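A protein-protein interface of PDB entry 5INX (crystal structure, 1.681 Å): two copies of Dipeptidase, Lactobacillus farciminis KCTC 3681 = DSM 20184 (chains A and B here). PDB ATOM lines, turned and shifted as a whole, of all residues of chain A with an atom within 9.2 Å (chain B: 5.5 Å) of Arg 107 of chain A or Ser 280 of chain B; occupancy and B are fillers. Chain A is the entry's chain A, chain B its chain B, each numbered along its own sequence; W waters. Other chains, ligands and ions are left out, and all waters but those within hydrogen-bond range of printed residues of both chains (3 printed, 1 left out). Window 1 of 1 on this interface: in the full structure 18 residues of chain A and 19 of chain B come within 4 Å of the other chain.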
ATOM      1  N   THR A 104     -16.404 -17.108  -5.547  1.00  0.00           N
ATOM      2  CA  THR A 104     -16.779 -17.592  -6.877  1.00  0.00           C
ATOM      3  C   THR A 104     -16.928 -16.379  -7.790  1.00  0.00           C
ATOM      4  O   THR A 104     -16.485 -15.288  -7.436  1.00  0.00           O
ATOM      5  CB  THR A 104     -18.085 -18.431  -6.816  1.00  0.00           C
ATOM      6  OG1 THR A 104     -18.360 -19.007  -8.097  1.00  0.00           O
ATOM      7  CG2 THR A 104     -19.273 -17.584  -6.365  1.00  0.00           C
ATOM      8  N   ASN A 105     -17.483 -16.552  -8.984  1.00  0.00           N
ATOM      9  CA  ASN A 105     -17.832 -15.383  -9.795  1.00  0.00           C
ATOM     10  C   ASN A 105     -19.046 -15.671 -10.673  1.00  0.00           C
ATOM     11  O   ASN A 105     -19.498 -16.809 -10.766  1.00  0.00           O
ATOM     12  CB  ASN A 105     -16.637 -14.893 -10.637  1.00  0.00           C
ATOM     13  CG  ASN A 105     -16.161 -15.901 -11.680  1.00  0.00           C
ATOM     14  OD1 ASN A 105     -16.902 -16.291 -12.581  1.00  0.00           O
ATOM     15  ND2 ASN A 105     -14.886 -16.267 -11.600  1.00  0.00           N
ATOM     16  N   SER A 106     -19.586 -14.620 -11.281  1.00  0.00           N
ATOM     17  CA  SER A 106     -20.851 -14.707 -11.999  1.00  0.00           C
ATOM     18  C   SER A 106     -20.751 -15.497 -13.299  1.00  0.00           C
ATOM     19  O   SER A 106     -21.749 -16.046 -13.765  1.00  0.00           O
ATOM     20  CB  SER A 106     -21.379 -13.304 -12.298  1.00  0.00           C
ATOM     21  OG  SER A 106     -20.366 -12.501 -12.883  1.00  0.00           O
ATOM     22  N   ARG A 107     -19.559 -15.544 -13.890  1.00  0.00           N
ATOM     23  CA  ARG A 107     -19.394 -16.234 -15.169  1.00  0.00           C
ATOM     24  C   ARG A 107     -19.535 -17.745 -14.974  1.00  0.00           C
ATOM     25  O   ARG A 107     -20.224 -18.418 -15.753  1.00  0.00           O
ATOM     26  CB  ARG A 107     -18.044 -15.869 -15.809  1.00  0.00           C
ATOM     27  CG  ARG A 107     -17.986 -14.413 -16.311  1.00  0.00           C
ATOM     28  CD  ARG A 107     -16.570 -13.934 -16.681  1.00  0.00           C
ATOM     29  NE  ARG A 107     -15.638 -14.013 -15.556  1.00  0.00           N
ATOM     30  CZ  ARG A 107     -15.614 -13.145 -14.549  1.00  0.00           C
ATOM     31  NH1 ARG A 107     -16.477 -12.134 -14.527  1.00  0.00           N
ATOM     32  NH2 ARG A 107     -14.739 -13.291 -13.554  1.00  0.00           N
ATOM     33  N   VAL A 108     -18.927 -18.293 -13.927  1.00  0.00           N
ATOM     34  CA  VAL A 108     -19.089 -19.726 -13.704  1.00  0.00           C
ATOM     35  C   VAL A 108     -20.454 -20.018 -13.072  1.00  0.00           C
ATOM     36  O   VAL A 108     -21.076 -21.042 -13.392  1.00  0.00           O
ATOM     37  CB  VAL A 108     -17.935 -20.327 -12.854  1.00  0.00           C
ATOM     38  CG1 VAL A 108     -17.839 -19.668 -11.489  1.00  0.00           C
ATOM     39  CG2 VAL A 108     -18.077 -21.855 -12.737  1.00  0.00           C
ATOM     40  N   GLN A 109     -20.951 -19.130 -12.208  1.00  0.00           N
ATOM     41  CA  GLN A 109     -22.269 -19.341 -11.608  1.00  0.00           C
ATOM     42  C   GLN A 109     -23.370 -19.338 -12.669  1.00  0.00           C
ATOM     43  O   GLN A 109     -24.381 -20.023 -12.523  1.00  0.00           O
ATOM     44  CB  GLN A 109     -22.580 -18.282 -10.532  1.00  0.00           C
ATOM     45  CG  GLN A 109     -21.772 -18.436  -9.241  1.00  0.00           C
ATOM     46  CD  GLN A 109     -22.088 -19.723  -8.495  1.00  0.00           C
ATOM     47  OE1 GLN A 109     -23.235 -20.161  -8.453  1.00  0.00           O
ATOM     48  NE2 GLN A 109     -21.062 -20.343  -7.912  1.00  0.00           N
ATOM     49  N   GLY A 110     -23.161 -18.582 -13.746  1.00  0.00           N
ATOM     50  CA  GLY A 110     -24.125 -18.542 -14.831  1.00  0.00           C
ATOM     51  C   GLY A 110     -24.197 -19.846 -15.608  1.00  0.00           C
ATOM     52  O   GLY A 110     -25.207 -20.136 -16.258  1.00  0.00           O
ATOM     53  N   LEU A 111     -23.137 -20.648 -15.525  1.00  0.00           N
ATOM     54  CA  LEU A 111     -23.076 -21.924 -16.249  1.00  0.00           C
ATOM     55  C   LEU A 111     -23.457 -23.121 -15.386  1.00  0.00           C
ATOM     56  O   LEU A 111     -24.047 -24.080 -15.874  1.00  0.00           O
ATOM     57  CB  LEU A 111     -21.677 -22.136 -16.820  1.00  0.00           C
ATOM     58  CG  LEU A 111     -21.299 -21.195 -17.961  1.00  0.00           C
ATOM     59  CD1 LEU A 111     -19.797 -21.226 -18.193  1.00  0.00           C
ATOM     60  CD2 LEU A 111     -22.048 -21.579 -19.236  1.00  0.00           C
ATOM     61  N   ASP A 112     -23.102 -23.056 -14.106  1.00  0.00           N
ATOM     62  CA  ASP A 112     -23.337 -24.145 -13.164  1.00  0.00           C
ATOM     63  C   ASP A 112     -23.785 -23.543 -11.830  1.00  0.00           C
ATOM     64  O   ASP A 112     -23.009 -23.474 -10.885  1.00  0.00           O
ATOM     65  CB  ASP A 112     -22.067 -24.996 -13.002  1.00  0.00           C
ATOM     66  CG  ASP A 112     -22.243 -26.164 -12.031  1.00  0.00           C
ATOM     67  OD1 ASP A 112     -23.392 -26.502 -11.687  1.00  0.00           O
ATOM     68  OD2 ASP A 112     -21.220 -26.748 -11.609  1.00  0.00           O
ATOM     69  N   PRO A 113     -25.051 -23.108 -11.759  1.00  0.00           N
ATOM     70  CA  PRO A 113     -25.582 -22.438 -10.564  1.00  0.00           C
ATOM     71  C   PRO A 113     -25.607 -23.332  -9.336  1.00  0.00           C
ATOM     72  O   PRO A 113     -25.604 -24.559  -9.456  1.00  0.00           O
ATOM     73  CB  PRO A 113     -27.019 -22.079 -10.969  1.00  0.00           C
ATOM     74  CG  PRO A 113     -27.041 -22.157 -12.450  1.00  0.00           C
ATOM     75  CD  PRO A 113     -26.069 -23.221 -12.816  1.00  0.00           C
ATOM     76  N   ILE A 171     -16.690 -25.607  -7.087  1.00  0.00           N
ATOM     77  CA  ILE A 171     -16.791 -24.656  -8.180  1.00  0.00           C
ATOM     78  C   ILE A 171     -18.180 -24.762  -8.770  1.00  0.00           C
ATOM     79  O   ILE A 171     -18.515 -25.777  -9.385  1.00  0.00           O
ATOM     80  CB  ILE A 171     -15.727 -24.945  -9.258  1.00  0.00           C
ATOM     81  CG1 ILE A 171     -14.326 -24.733  -8.679  1.00  0.00           C
ATOM     82  CG2 ILE A 171     -15.940 -24.085 -10.488  1.00  0.00           C
ATOM     83  CD1 ILE A 171     -13.236 -25.380  -9.517  1.00  0.00           C
ATOM     84  N   GLY A 172     -19.005 -23.741  -8.561  1.00  0.00           N
ATOM     85  CA  GLY A 172     -20.395 -23.815  -8.984  1.00  0.00           C
ATOM     86  C   GLY A 172     -21.176 -24.904  -8.258  1.00  0.00           C
ATOM     87  O   GLY A 172     -20.803 -25.344  -7.168  1.00  0.00           O
ATOM     88  N   LEU A 214     -14.954 -27.179 -19.733  1.00  0.00           N
ATOM     89  CA  LEU A 214     -15.839 -26.129 -19.251  1.00  0.00           C
ATOM     90  C   LEU A 214     -15.188 -24.766 -19.444  1.00  0.00           C
ATOM     91  O   LEU A 214     -15.814 -23.817 -19.923  1.00  0.00           O
ATOM     92  CB  LEU A 214     -16.191 -26.338 -17.778  1.00  0.00           C
ATOM     93  CG  LEU A 214     -17.149 -25.290 -17.200  1.00  0.00           C
ATOM     94  CD1 LEU A 214     -18.570 -25.472 -17.746  1.00  0.00           C
ATOM     95  CD2 LEU A 214     -17.130 -25.339 -15.688  1.00  0.00           C
ATOM     96  N   ASN A 218     -16.247 -22.181 -22.914  1.00  0.00           N
ATOM     97  CA  ASN A 218     -17.110 -21.087 -22.481  1.00  0.00           C
ATOM     98  C   ASN A 218     -16.357 -19.786 -22.219  1.00  0.00           C
ATOM     99  O   ASN A 218     -16.896 -18.869 -21.596  1.00  0.00           O
ATOM    100  CB  ASN A 218     -17.883 -21.504 -21.231  1.00  0.00           C
ATOM    101  CG  ASN A 218     -18.840 -22.657 -21.509  1.00  0.00           C
ATOM    102  OD1 ASN A 218     -19.911 -22.458 -22.089  1.00  0.00           O
ATOM    103  ND2 ASN A 218     -18.438 -23.872 -21.139  1.00  0.00           N
ATOM    104  N   ASN A 219     -15.123 -19.717 -22.716  1.00  0.00           N
ATOM    105  CA  ASN A 219     -14.301 -18.515 -22.623  1.00  0.00           C
ATOM    106  C   ASN A 219     -14.187 -18.009 -21.192  1.00  0.00           C
ATOM    107  O   ASN A 219     -14.328 -16.815 -20.933  1.00  0.00           O
ATOM    108  CB  ASN A 219     -14.876 -17.414 -23.519  1.00  0.00           C
ATOM    109  CG  ASN A 219     -14.774 -17.756 -24.995  1.00  0.00           C
ATOM    110  OD1 ASN A 219     -13.752 -18.263 -25.458  1.00  0.00           O
ATOM    111  ND2 ASN A 219     -15.845 -17.498 -25.734  1.00  0.00           N
ATOM    112  N   LEU A 220     -13.943 -18.926 -20.263  1.00  0.00           N
ATOM    113  CA  LEU A 220     -13.850 -18.536 -18.858  1.00  0.00           C
ATOM    114  C   LEU A 220     -12.453 -18.061 -18.475  1.00  0.00           C
ATOM    115  O   LEU A 220     -12.273 -17.445 -17.418  1.00  0.00           O
ATOM    116  CB  LEU A 220     -14.245 -19.699 -17.942  1.00  0.00           C
ATOM    117  CG  LEU A 220     -15.682 -20.198 -18.071  1.00  0.00           C
ATOM    118  CD1 LEU A 220     -15.974 -21.313 -17.060  1.00  0.00           C
ATOM    119  CD2 LEU A 220     -16.671 -19.055 -17.913  1.00  0.00           C
ATOM    120  N   ASN A 221     -11.466 -18.358 -19.310  1.00  0.00           N
ATOM    121  CA  ASN A 221     -10.079 -18.099 -18.931  1.00  0.00           C
ATOM    122  C   ASN A 221      -9.653 -16.667 -19.226  1.00  0.00           C
ATOM    123  O   ASN A 221      -9.616 -16.259 -20.386  1.00  0.00           O
ATOM    124  CB  ASN A 221      -9.143 -19.083 -19.648  1.00  0.00           C
ATOM    125  CG  ASN A 221      -7.783 -19.186 -18.987  1.00  0.00           C
ATOM    126  OD1 ASN A 221      -7.344 -18.268 -18.284  1.00  0.00           O
ATOM    127  ND2 ASN A 221      -7.105 -20.311 -19.198  1.00  0.00           N
ATOM    128  N   PRO A 222      -9.328 -15.891 -18.175  1.00  0.00           N
ATOM    129  CA  PRO A 222      -8.938 -14.496 -18.407  1.00  0.00           C
ATOM    130  C   PRO A 222      -7.482 -14.336 -18.797  1.00  0.00           C
ATOM    131  O   PRO A 222      -7.069 -13.260 -19.232  1.00  0.00           O
ATOM    132  CB  PRO A 222      -9.198 -13.837 -17.049  1.00  0.00           C
ATOM    133  CG  PRO A 222      -8.918 -14.927 -16.069  1.00  0.00           C
ATOM    134  CD  PRO A 222      -9.392 -16.213 -16.738  1.00  0.00           C
ATOM    135  N   LEU A 229      -6.718 -21.399 -11.461  1.00  0.00           N
ATOM    136  CA  LEU A 229      -8.121 -21.691 -11.188  1.00  0.00           C
ATOM    137  C   LEU A 229      -8.849 -20.552 -10.484  1.00  0.00           C
ATOM    138  O   LEU A 229     -10.019 -20.329 -10.768  1.00  0.00           O
ATOM    139  CB  LEU A 229      -8.270 -22.977 -10.377  1.00  0.00           C
ATOM    140  CG  LEU A 229      -7.885 -24.257 -11.125  1.00  0.00           C
ATOM    141  CD1 LEU A 229      -8.490 -25.449 -10.445  1.00  0.00           C
ATOM    142  CD2 LEU A 229      -8.297 -24.210 -12.604  1.00  0.00           C
ATOM    143  N   ARG A 230      -8.185 -19.823  -9.589  1.00  0.00           N
ATOM    144  CA  ARG A 230      -8.896 -18.743  -8.904  1.00  0.00           C
ATOM    145  C   ARG A 230      -9.037 -17.514  -9.818  1.00  0.00           C
ATOM    146  O   ARG A 230      -9.993 -16.756  -9.691  1.00  0.00           O
ATOM    147  CB  ARG A 230      -8.219 -18.392  -7.577  1.00  0.00           C
ATOM    148  CG  ARG A 230      -6.895 -17.680  -7.672  1.00  0.00           C
ATOM    149  CD  ARG A 230      -6.122 -17.901  -6.372  1.00  0.00           C
ATOM    150  NE  ARG A 230      -5.282 -16.750  -6.073  1.00  0.00           N
ATOM    151  CZ  ARG A 230      -4.349 -16.714  -5.123  1.00  0.00           C
ATOM    152  NH1 ARG A 230      -4.085 -17.776  -4.374  1.00  0.00           N
ATOM    153  NH2 ARG A 230      -3.659 -15.601  -4.934  1.00  0.00           N
ATOM    154  N   HIS A 231      -8.121 -17.346 -10.769  1.00  0.00           N
ATOM    155  CA  HIS A 231      -8.323 -16.347 -11.814  1.00  0.00           C
ATOM    156  C   HIS A 231      -9.584 -16.667 -12.613  1.00  0.00           C
ATOM    157  O   HIS A 231     -10.372 -15.792 -12.955  1.00  0.00           O
ATOM    158  CB  HIS A 231      -7.125 -16.300 -12.766  1.00  0.00           C
ATOM    159  CG  HIS A 231      -5.932 -15.598 -12.205  1.00  0.00           C
ATOM    160  ND1 HIS A 231      -4.811 -15.327 -12.955  1.00  0.00           N
ATOM    161  CD2 HIS A 231      -5.692 -15.097 -10.969  1.00  0.00           C
ATOM    162  CE1 HIS A 231      -3.923 -14.695 -12.204  1.00  0.00           C
ATOM    163  NE2 HIS A 231      -4.435 -14.544 -10.996  1.00  0.00           N
ATOM    164  N   ILE A 232      -9.776 -17.950 -12.883  1.00  0.00           N
ATOM    165  CA  ILE A 232     -10.875 -18.405 -13.728  1.00  0.00           C
ATOM    166  C   ILE A 232     -12.211 -18.485 -12.992  1.00  0.00           C
ATOM    167  O   ILE A 232     -13.247 -18.025 -13.502  1.00  0.00           O
ATOM    168  CB  ILE A 232     -10.540 -19.789 -14.322  1.00  0.00           C
ATOM    169  CG1 ILE A 232      -9.289 -19.677 -15.205  1.00  0.00           C
ATOM    170  CG2 ILE A 232     -11.753 -20.373 -15.091  1.00  0.00           C
ATOM    171  CD1 ILE A 232      -8.661 -21.020 -15.551  1.00  0.00           C
ATOM    172  N   PHE A 233     -12.180 -19.062 -11.792  1.00  0.00           N
ATOM    173  CA  PHE A 233     -13.400 -19.440 -11.083  1.00  0.00           C
ATOM    174  C   PHE A 233     -13.615 -18.626  -9.808  1.00  0.00           C
ATOM    175  O   PHE A 233     -14.667 -18.723  -9.163  1.00  0.00           O
ATOM    176  CB  PHE A 233     -13.358 -20.922 -10.708  1.00  0.00           C
ATOM    177  CG  PHE A 233     -13.395 -21.871 -11.884  1.00  0.00           C
ATOM    178  CD1 PHE A 233     -14.478 -21.889 -12.746  1.00  0.00           C
ATOM    179  CD2 PHE A 233     -12.381 -22.797 -12.064  1.00  0.00           C
ATOM    180  CE1 PHE A 233     -14.536 -22.799 -13.805  1.00  0.00           C
ATOM    181  CE2 PHE A 233     -12.426 -23.708 -13.120  1.00  0.00           C
ATOM    182  CZ  PHE A 233     -13.507 -23.707 -13.981  1.00  0.00           C
ATOM    183  N   GLY A 234     -12.614 -17.838  -9.434  1.00  0.00           N
ATOM    184  CA  GLY A 234     -12.656 -17.164  -8.147  1.00  0.00           C
ATOM    185  C   GLY A 234     -12.848 -15.668  -8.244  1.00  0.00           C
ATOM    186  O   GLY A 234     -13.465 -15.153  -9.184  1.00  0.00           O
ATOM    187  N   SER A 235     -12.319 -14.966  -7.251  1.00  0.00           N
ATOM    188  CA  SER A 235     -12.470 -13.523  -7.166  1.00  0.00           C
ATOM    189  C   SER A 235     -11.121 -12.842  -6.956  1.00  0.00           C
ATOM    190  O   SER A 235     -10.166 -13.455  -6.464  1.00  0.00           O
ATOM    191  CB  SER A 235     -13.418 -13.158  -6.021  1.00  0.00           C
ATOM    192  OG  SER A 235     -12.865 -13.546  -4.774  1.00  0.00           O
ATOM    193  N   ALA A 236     -11.059 -11.576  -7.359  1.00  0.00           N
ATOM    194  CA  ALA A 236      -9.982 -10.665  -6.972  1.00  0.00           C
ATOM    195  C   ALA A 236     -10.629  -9.308  -6.755  1.00  0.00           C
ATOM    196  O   ALA A 236     -10.452  -8.377  -7.541  1.00  0.00           O
ATOM    197  CB  ALA A 236      -8.893 -10.603  -8.034  1.00  0.00           C
ATOM    198  N   ILE B  20     -12.449 -11.067 -22.790  1.00  0.00           N
ATOM    199  CA  ILE B  20     -12.366 -12.443 -22.349  1.00  0.00           C
ATOM    200  C   ILE B  20     -13.086 -13.379 -23.323  1.00  0.00           C
ATOM    201  O   ILE B  20     -12.737 -14.554 -23.421  1.00  0.00           O
ATOM    202  CB  ILE B  20     -12.947 -12.606 -20.921  1.00  0.00           C
ATOM    203  CG1 ILE B  20     -12.477 -13.924 -20.302  1.00  0.00           C
ATOM    204  CG2 ILE B  20     -14.469 -12.459 -20.927  1.00  0.00           C
ATOM    205  CD1 ILE B  20     -12.817 -14.052 -18.798  1.00  0.00           C
ATOM    206  N   LEU B  25     -16.104  -4.297 -27.133  1.00  0.00           N
ATOM    207  CA  LEU B  25     -16.843  -3.544 -26.118  1.00  0.00           C
ATOM    208  C   LEU B  25     -16.584  -2.051 -26.241  1.00  0.00           C
ATOM    209  O   LEU B  25     -15.434  -1.624 -26.321  1.00  0.00           O
ATOM    210  CB  LEU B  25     -16.456  -3.988 -24.695  1.00  0.00           C
ATOM    211  CG  LEU B  25     -16.568  -5.447 -24.260  1.00  0.00           C
ATOM    212  CD1 LEU B  25     -15.874  -5.631 -22.905  1.00  0.00           C
ATOM    213  CD2 LEU B  25     -18.018  -5.865 -24.163  1.00  0.00           C
ATOM    214  N   LYS B 278      -7.152 -10.738 -20.112  1.00  0.00           N
ATOM    215  CA  LYS B 278      -8.326 -10.411 -20.900  1.00  0.00           C
ATOM    216  C   LYS B 278      -9.393  -9.774 -20.020  1.00  0.00           C
ATOM    217  O   LYS B 278      -9.491 -10.055 -18.813  1.00  0.00           O
ATOM    218  CB  LYS B 278      -8.878 -11.649 -21.596  1.00  0.00           C
ATOM    219  CG  LYS B 278      -7.893 -12.296 -22.549  1.00  0.00           C
ATOM    220  CD  LYS B 278      -8.495 -13.587 -23.105  1.00  0.00           C
ATOM    221  CE  LYS B 278      -7.552 -14.317 -24.045  1.00  0.00           C
ATOM    222  NZ  LYS B 278      -8.192 -15.584 -24.538  1.00  0.00           N
ATOM    223  N   ILE B 279     -10.189  -8.913 -20.644  1.00  0.00           N
ATOM    224  CA  ILE B 279     -11.123  -8.041 -19.936  1.00  0.00           C
ATOM    225  C   ILE B 279     -12.573  -8.526 -20.036  1.00  0.00           C
ATOM    226  O   ILE B 279     -13.056  -8.859 -21.119  1.00  0.00           O
ATOM    227  CB  ILE B 279     -10.994  -6.615 -20.490  1.00  0.00           C
ATOM    228  CG1 ILE B 279      -9.560  -6.110 -20.268  1.00  0.00           C
ATOM    229  CG2 ILE B 279     -12.051  -5.683 -19.901  1.00  0.00           C
ATOM    230  CD1 ILE B 279      -9.275  -4.787 -20.952  1.00  0.00           C
ATOM    231  N   SER B 280     -13.256  -8.571 -18.895  1.00  0.00           N
ATOM    232  CA  SER B 280     -14.645  -9.021 -18.830  1.00  0.00           C
ATOM    233  C   SER B 280     -15.582  -7.838 -18.714  1.00  0.00           C
ATOM    234  O   SER B 280     -15.152  -6.731 -18.403  1.00  0.00           O
ATOM    235  CB  SER B 280     -14.860  -9.945 -17.628  1.00  0.00           C
ATOM    236  OG  SER B 280     -14.779  -9.194 -16.423  1.00  0.00           O
ATOM    237  N   VAL B 281     -16.869  -8.077 -18.926  1.00  0.00           N
ATOM    238  CA  VAL B 281     -17.871  -7.034 -18.738  1.00  0.00           C
ATOM    239  C   VAL B 281     -17.874  -6.611 -17.271  1.00  0.00           C
ATOM    240  O   VAL B 281     -17.961  -5.423 -16.958  1.00  0.00           O
ATOM    241  CB  VAL B 281     -19.277  -7.505 -19.182  1.00  0.00           C
ATOM    242  CG1 VAL B 281     -20.364  -6.555 -18.689  1.00  0.00           C
ATOM    243  CG2 VAL B 281     -19.335  -7.607 -20.712  1.00  0.00           C
ATOM    244  N   GLU B 282     -17.744  -7.589 -16.381  1.00  0.00           N
ATOM    245  CA  GLU B 282     -17.635  -7.302 -14.952  1.00  0.00           C
ATOM    246  C   GLU B 282     -16.472  -6.336 -14.645  1.00  0.00           C
ATOM    247  O   GLU B 282     -16.634  -5.405 -13.840  1.00  0.00           O
ATOM    248  CB  GLU B 282     -17.475  -8.606 -14.162  1.00  0.00           C
ATOM    249  CG  GLU B 282     -18.757  -9.457 -14.033  1.00  0.00           C
ATOM    250  CD  GLU B 282     -19.066 -10.404 -15.226  1.00  0.00           C
ATOM    251  OE1 GLU B 282     -18.323 -10.456 -16.257  1.00  0.00           O
ATOM    252  OE2 GLU B 282     -20.091 -11.136 -15.100  1.00  0.00           O
ATOM    253  N   ASP B 283     -15.316  -6.558 -15.282  1.00  0.00           N
ATOM    254  CA  ASP B 283     -14.156  -5.654 -15.162  1.00  0.00           C
ATOM    255  C   ASP B 283     -14.487  -4.223 -15.577  1.00  0.00           C
ATOM    256  O   ASP B 283     -14.131  -3.270 -14.892  1.00  0.00           O
ATOM    257  CB  ASP B 283     -12.981  -6.122 -16.029  1.00  0.00           C
ATOM    258  CG  ASP B 283     -12.333  -7.389 -15.530  1.00  0.00           C
ATOM    259  OD1 ASP B 283     -12.413  -7.680 -14.314  1.00  0.00           O
ATOM    260  OD2 ASP B 283     -11.719  -8.087 -16.374  1.00  0.00           O
ATOM    261  N   VAL B 284     -15.123  -4.080 -16.732  1.00  0.00           N
ATOM    262  CA  VAL B 284     -15.482  -2.762 -17.234  1.00  0.00           C
ATOM    263  C   VAL B 284     -16.441  -2.061 -16.271  1.00  0.00           C
ATOM    264  O   VAL B 284     -16.257  -0.884 -15.958  1.00  0.00           O
ATOM    265  CB  VAL B 284     -16.103  -2.860 -18.636  1.00  0.00           C
ATOM    266  CG1 VAL B 284     -16.630  -1.510 -19.068  1.00  0.00           C
ATOM    267  CG2 VAL B 284     -15.061  -3.374 -19.617  1.00  0.00           C
ATOM    268  N   LYS B 285     -17.460  -2.773 -15.790  1.00  0.00           N
ATOM    269  CA  LYS B 285     -18.421  -2.164 -14.857  1.00  0.00           C
ATOM    270  C   LYS B 285     -17.732  -1.753 -13.558  1.00  0.00           C
ATOM    271  O   LYS B 285     -18.025  -0.686 -13.006  1.00  0.00           O
ATOM    272  CB  LYS B 285     -19.600  -3.115 -14.585  1.00  0.00           C
ATOM    273  CG  LYS B 285     -20.648  -2.617 -13.566  1.00  0.00           C
ATOM    274  CD  LYS B 285     -21.240  -1.239 -13.952  1.00  0.00           C
ATOM    275  CE  LYS B 285     -22.507  -0.940 -13.153  1.00  0.00           C
ATOM    276  NZ  LYS B 285     -22.298  -0.957 -11.652  1.00  0.00           N
ATOM    277  N   ARG B 411     -26.515 -13.915 -16.276  1.00  0.00           N
ATOM    278  CA  ARG B 411     -25.714 -14.779 -17.129  1.00  0.00           C
ATOM    279  C   ARG B 411     -26.401 -16.123 -17.345  1.00  0.00           C
ATOM    280  O   ARG B 411     -26.302 -16.695 -18.420  1.00  0.00           O
ATOM    281  CB  ARG B 411     -24.315 -14.970 -16.546  1.00  0.00           C
ATOM    282  CG  ARG B 411     -23.460 -13.696 -16.620  1.00  0.00           C
ATOM    283  CD  ARG B 411     -22.058 -14.016 -17.110  1.00  0.00           C
ATOM    284  NE  ARG B 411     -21.204 -12.843 -17.304  1.00  0.00           N
ATOM    285  CZ  ARG B 411     -20.942 -12.279 -18.483  1.00  0.00           C
ATOM    286  NH1 ARG B 411     -21.494 -12.746 -19.595  1.00  0.00           N
ATOM    287  NH2 ARG B 411     -20.120 -11.236 -18.549  1.00  0.00           N
ATOM    288  N   ASN B 415     -27.193 -17.408 -20.963  1.00  0.00           N
ATOM    289  CA  ASN B 415     -26.704 -18.720 -21.396  1.00  0.00           C
ATOM    290  C   ASN B 415     -27.842 -19.628 -21.867  1.00  0.00           C
ATOM    291  O   ASN B 415     -27.711 -20.320 -22.873  1.00  0.00           O
ATOM    292  CB  ASN B 415     -25.914 -19.398 -20.270  1.00  0.00           C
ATOM    293  CG  ASN B 415     -24.586 -18.711 -19.998  1.00  0.00           C
ATOM    294  OD1 ASN B 415     -24.004 -18.087 -20.889  1.00  0.00           O
ATOM    295  ND2 ASN B 415     -24.108 -18.804 -18.752  1.00  0.00           N
HETATM  296  O   HOH W   1     -13.627 -10.239 -14.246  1.00  0.00           O
HETATM  297  O   HOH W   2     -10.913 -16.540 -22.757  1.00  0.00           O
HETATM  298  O   HOH W   3      -7.611 -17.357 -22.425  1.00  0.00           O
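The side-chain hydroxyl of Ser 106 of chain A lies within hydrogen-bond range of the side-chain carboxylate of Glu 282 of chain B (2.6 Å).
The backbone carbonyl oxygen of Pro 222 of chain A lies within hydrogen-bond range of the backbone NH of Lys 278 of chain B (2.7 Å).
NH1 of Arg 107 of chain A is in salt-bridge range of OE1 of Glu 282 of chain B.
The backbone carbonyl oxygen (O) of Gly 110 of chain A sits at hydrogen-bond distance from the side-chain amide nitrogen (ND2) of Asn 415 of chain B (3.0 Å).
The side-chain carboxylate (OE2) of Glu 282 of chain B lies within salt-bridge range of the guanidinium group (NE) of Arg 411 of chain B, at 3.0 Å.
The side-chain hydroxyl (OG) of Ser 280 of chain B lies close to the backbone NH (N) of Glu 282 of chain B (3.4 Å).
The side-chain amide oxygen of Asn 105 of chain A is in hydrogen-bond range of the backbone NH of Arg 107 of chain A, 3.1 Å away.
OG of Ser 280 of chain B lies within hydrogen-bond range of N of Asp 283 of chain B, at 2.9 Å.
O of Arg 411 of chain B sits at hydrogen-bond distance from ND2 of Asn 415 of chain B, 3.1 Å away.
Ser 106 of chain A touches Arg 411 of chain B.
OG of Ser 280 of chain B touches NH1 of Arg 107 of chain A, 3.9 Å away.
Arg 107 of chain A touches Arg 411 of chain B.
Gly 110 of chain A touches Arg 411 of chain B (CA to CB, 3.97 Å).
CD2 of Leu 111 of chain A touches ND2 of Asn 415 of chain B (3.5 Å).
Asn 219 of chain A touches Ile 20 of chain B (O to CG1, 3.5 Å).
Ile 20 of chain B touches Leu 220 of chain A (CD1 to O, 3.7 Å).
Ile 20 of chain B touches Asn 221 of chain A (CG1 to O, 3.7 Å).
Asn 221 of chain A touches Lys 278 of chain B.
CD1 of Ile 20 of chain B touches CA of Pro 222 of chain A, at 3.9 Å.
Arg 107 of chain A touches three residues of chain B.
Printed residues of chain B within 4 Å of Gly 110 of chain A: Arg 411 (3.97 Å) and Asn 415 (3.0 Å).
Printed residues of chain A within 4 Å of Ile 20 of chain B: Asn 219, Leu 220, Asn 221 and Pro 222.
Printed residues of chain A within 4 Å of Lys 278 of chain B: Asn 221 (3.97 Å) and Pro 222 (2.7 Å).
Of chain A, only Arg 107 (3.9 Å) comes within 4 Å of Ser 280 of chain B.
Glu 282 of chain B touches two residues of chain A.
No residue of chain A comes within 4 Å of Asp 283 of chain B.
Of the printed residues of chain A, Asn 415 of chain B touches Gly 110 (3.0 Å) and Leu 111 (3.5 Å).
The nearest residue of chain B that does not touch Arg 107 of chain A is Ile 20 of chain B (4.3 Å).
The nearest residue of chain A that does not touch Ser 280 of chain B is Pro 222 of chain A (6.9 Å).
Of the 12 printed residues of chain B, 6 touch a printed residue of chain A.
Printed residues of chain B that touch a printed residue of chain A: Ile 20, Lys 278, Ser 280, Glu 282, Arg 411 and Asn 415.
Hydrophobic or aromatic side chains of chain A within 4 Å of the printed part of chain B: Leu 111.
Among the printed residues, Asp or Glu carboxylates within 4 Å of a Lys or Arg side-chain nitrogen of the other chain: Arg 107 of chain A with Glu 282 of chain B (3.0 Å).
No position is printed for both chains.
Of the 14 pairs that touch across the chains among the printed residues, none has its exchanged pair printed and touching as well.
Water W1 lies within hydrogen-bond range of the side-chain hydroxyl (OG) of Ser 280 of chain B (2.7 Å), the side-chain carboxylate (OD1) of Asp 283 of chain B (2.8 Å) and the guanidinium group (NH2) of Arg 107 of chain A (3.3 Å).
Water W2 lies within hydrogen-bond range of the backbone carbonyl oxygen of Asn 221 of chain A (2.7 Å), the backbone carbonyl oxygen of Ile 20 of chain B (2.8 Å) and the side-chain amino group of Lys 278 of chain B (3.4 Å).
Water W3 lies within hydrogen-bond range of NZ of Lys 278 of chain B (2.8 Å) and O of Asn 221 of chain A (3.1 Å).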
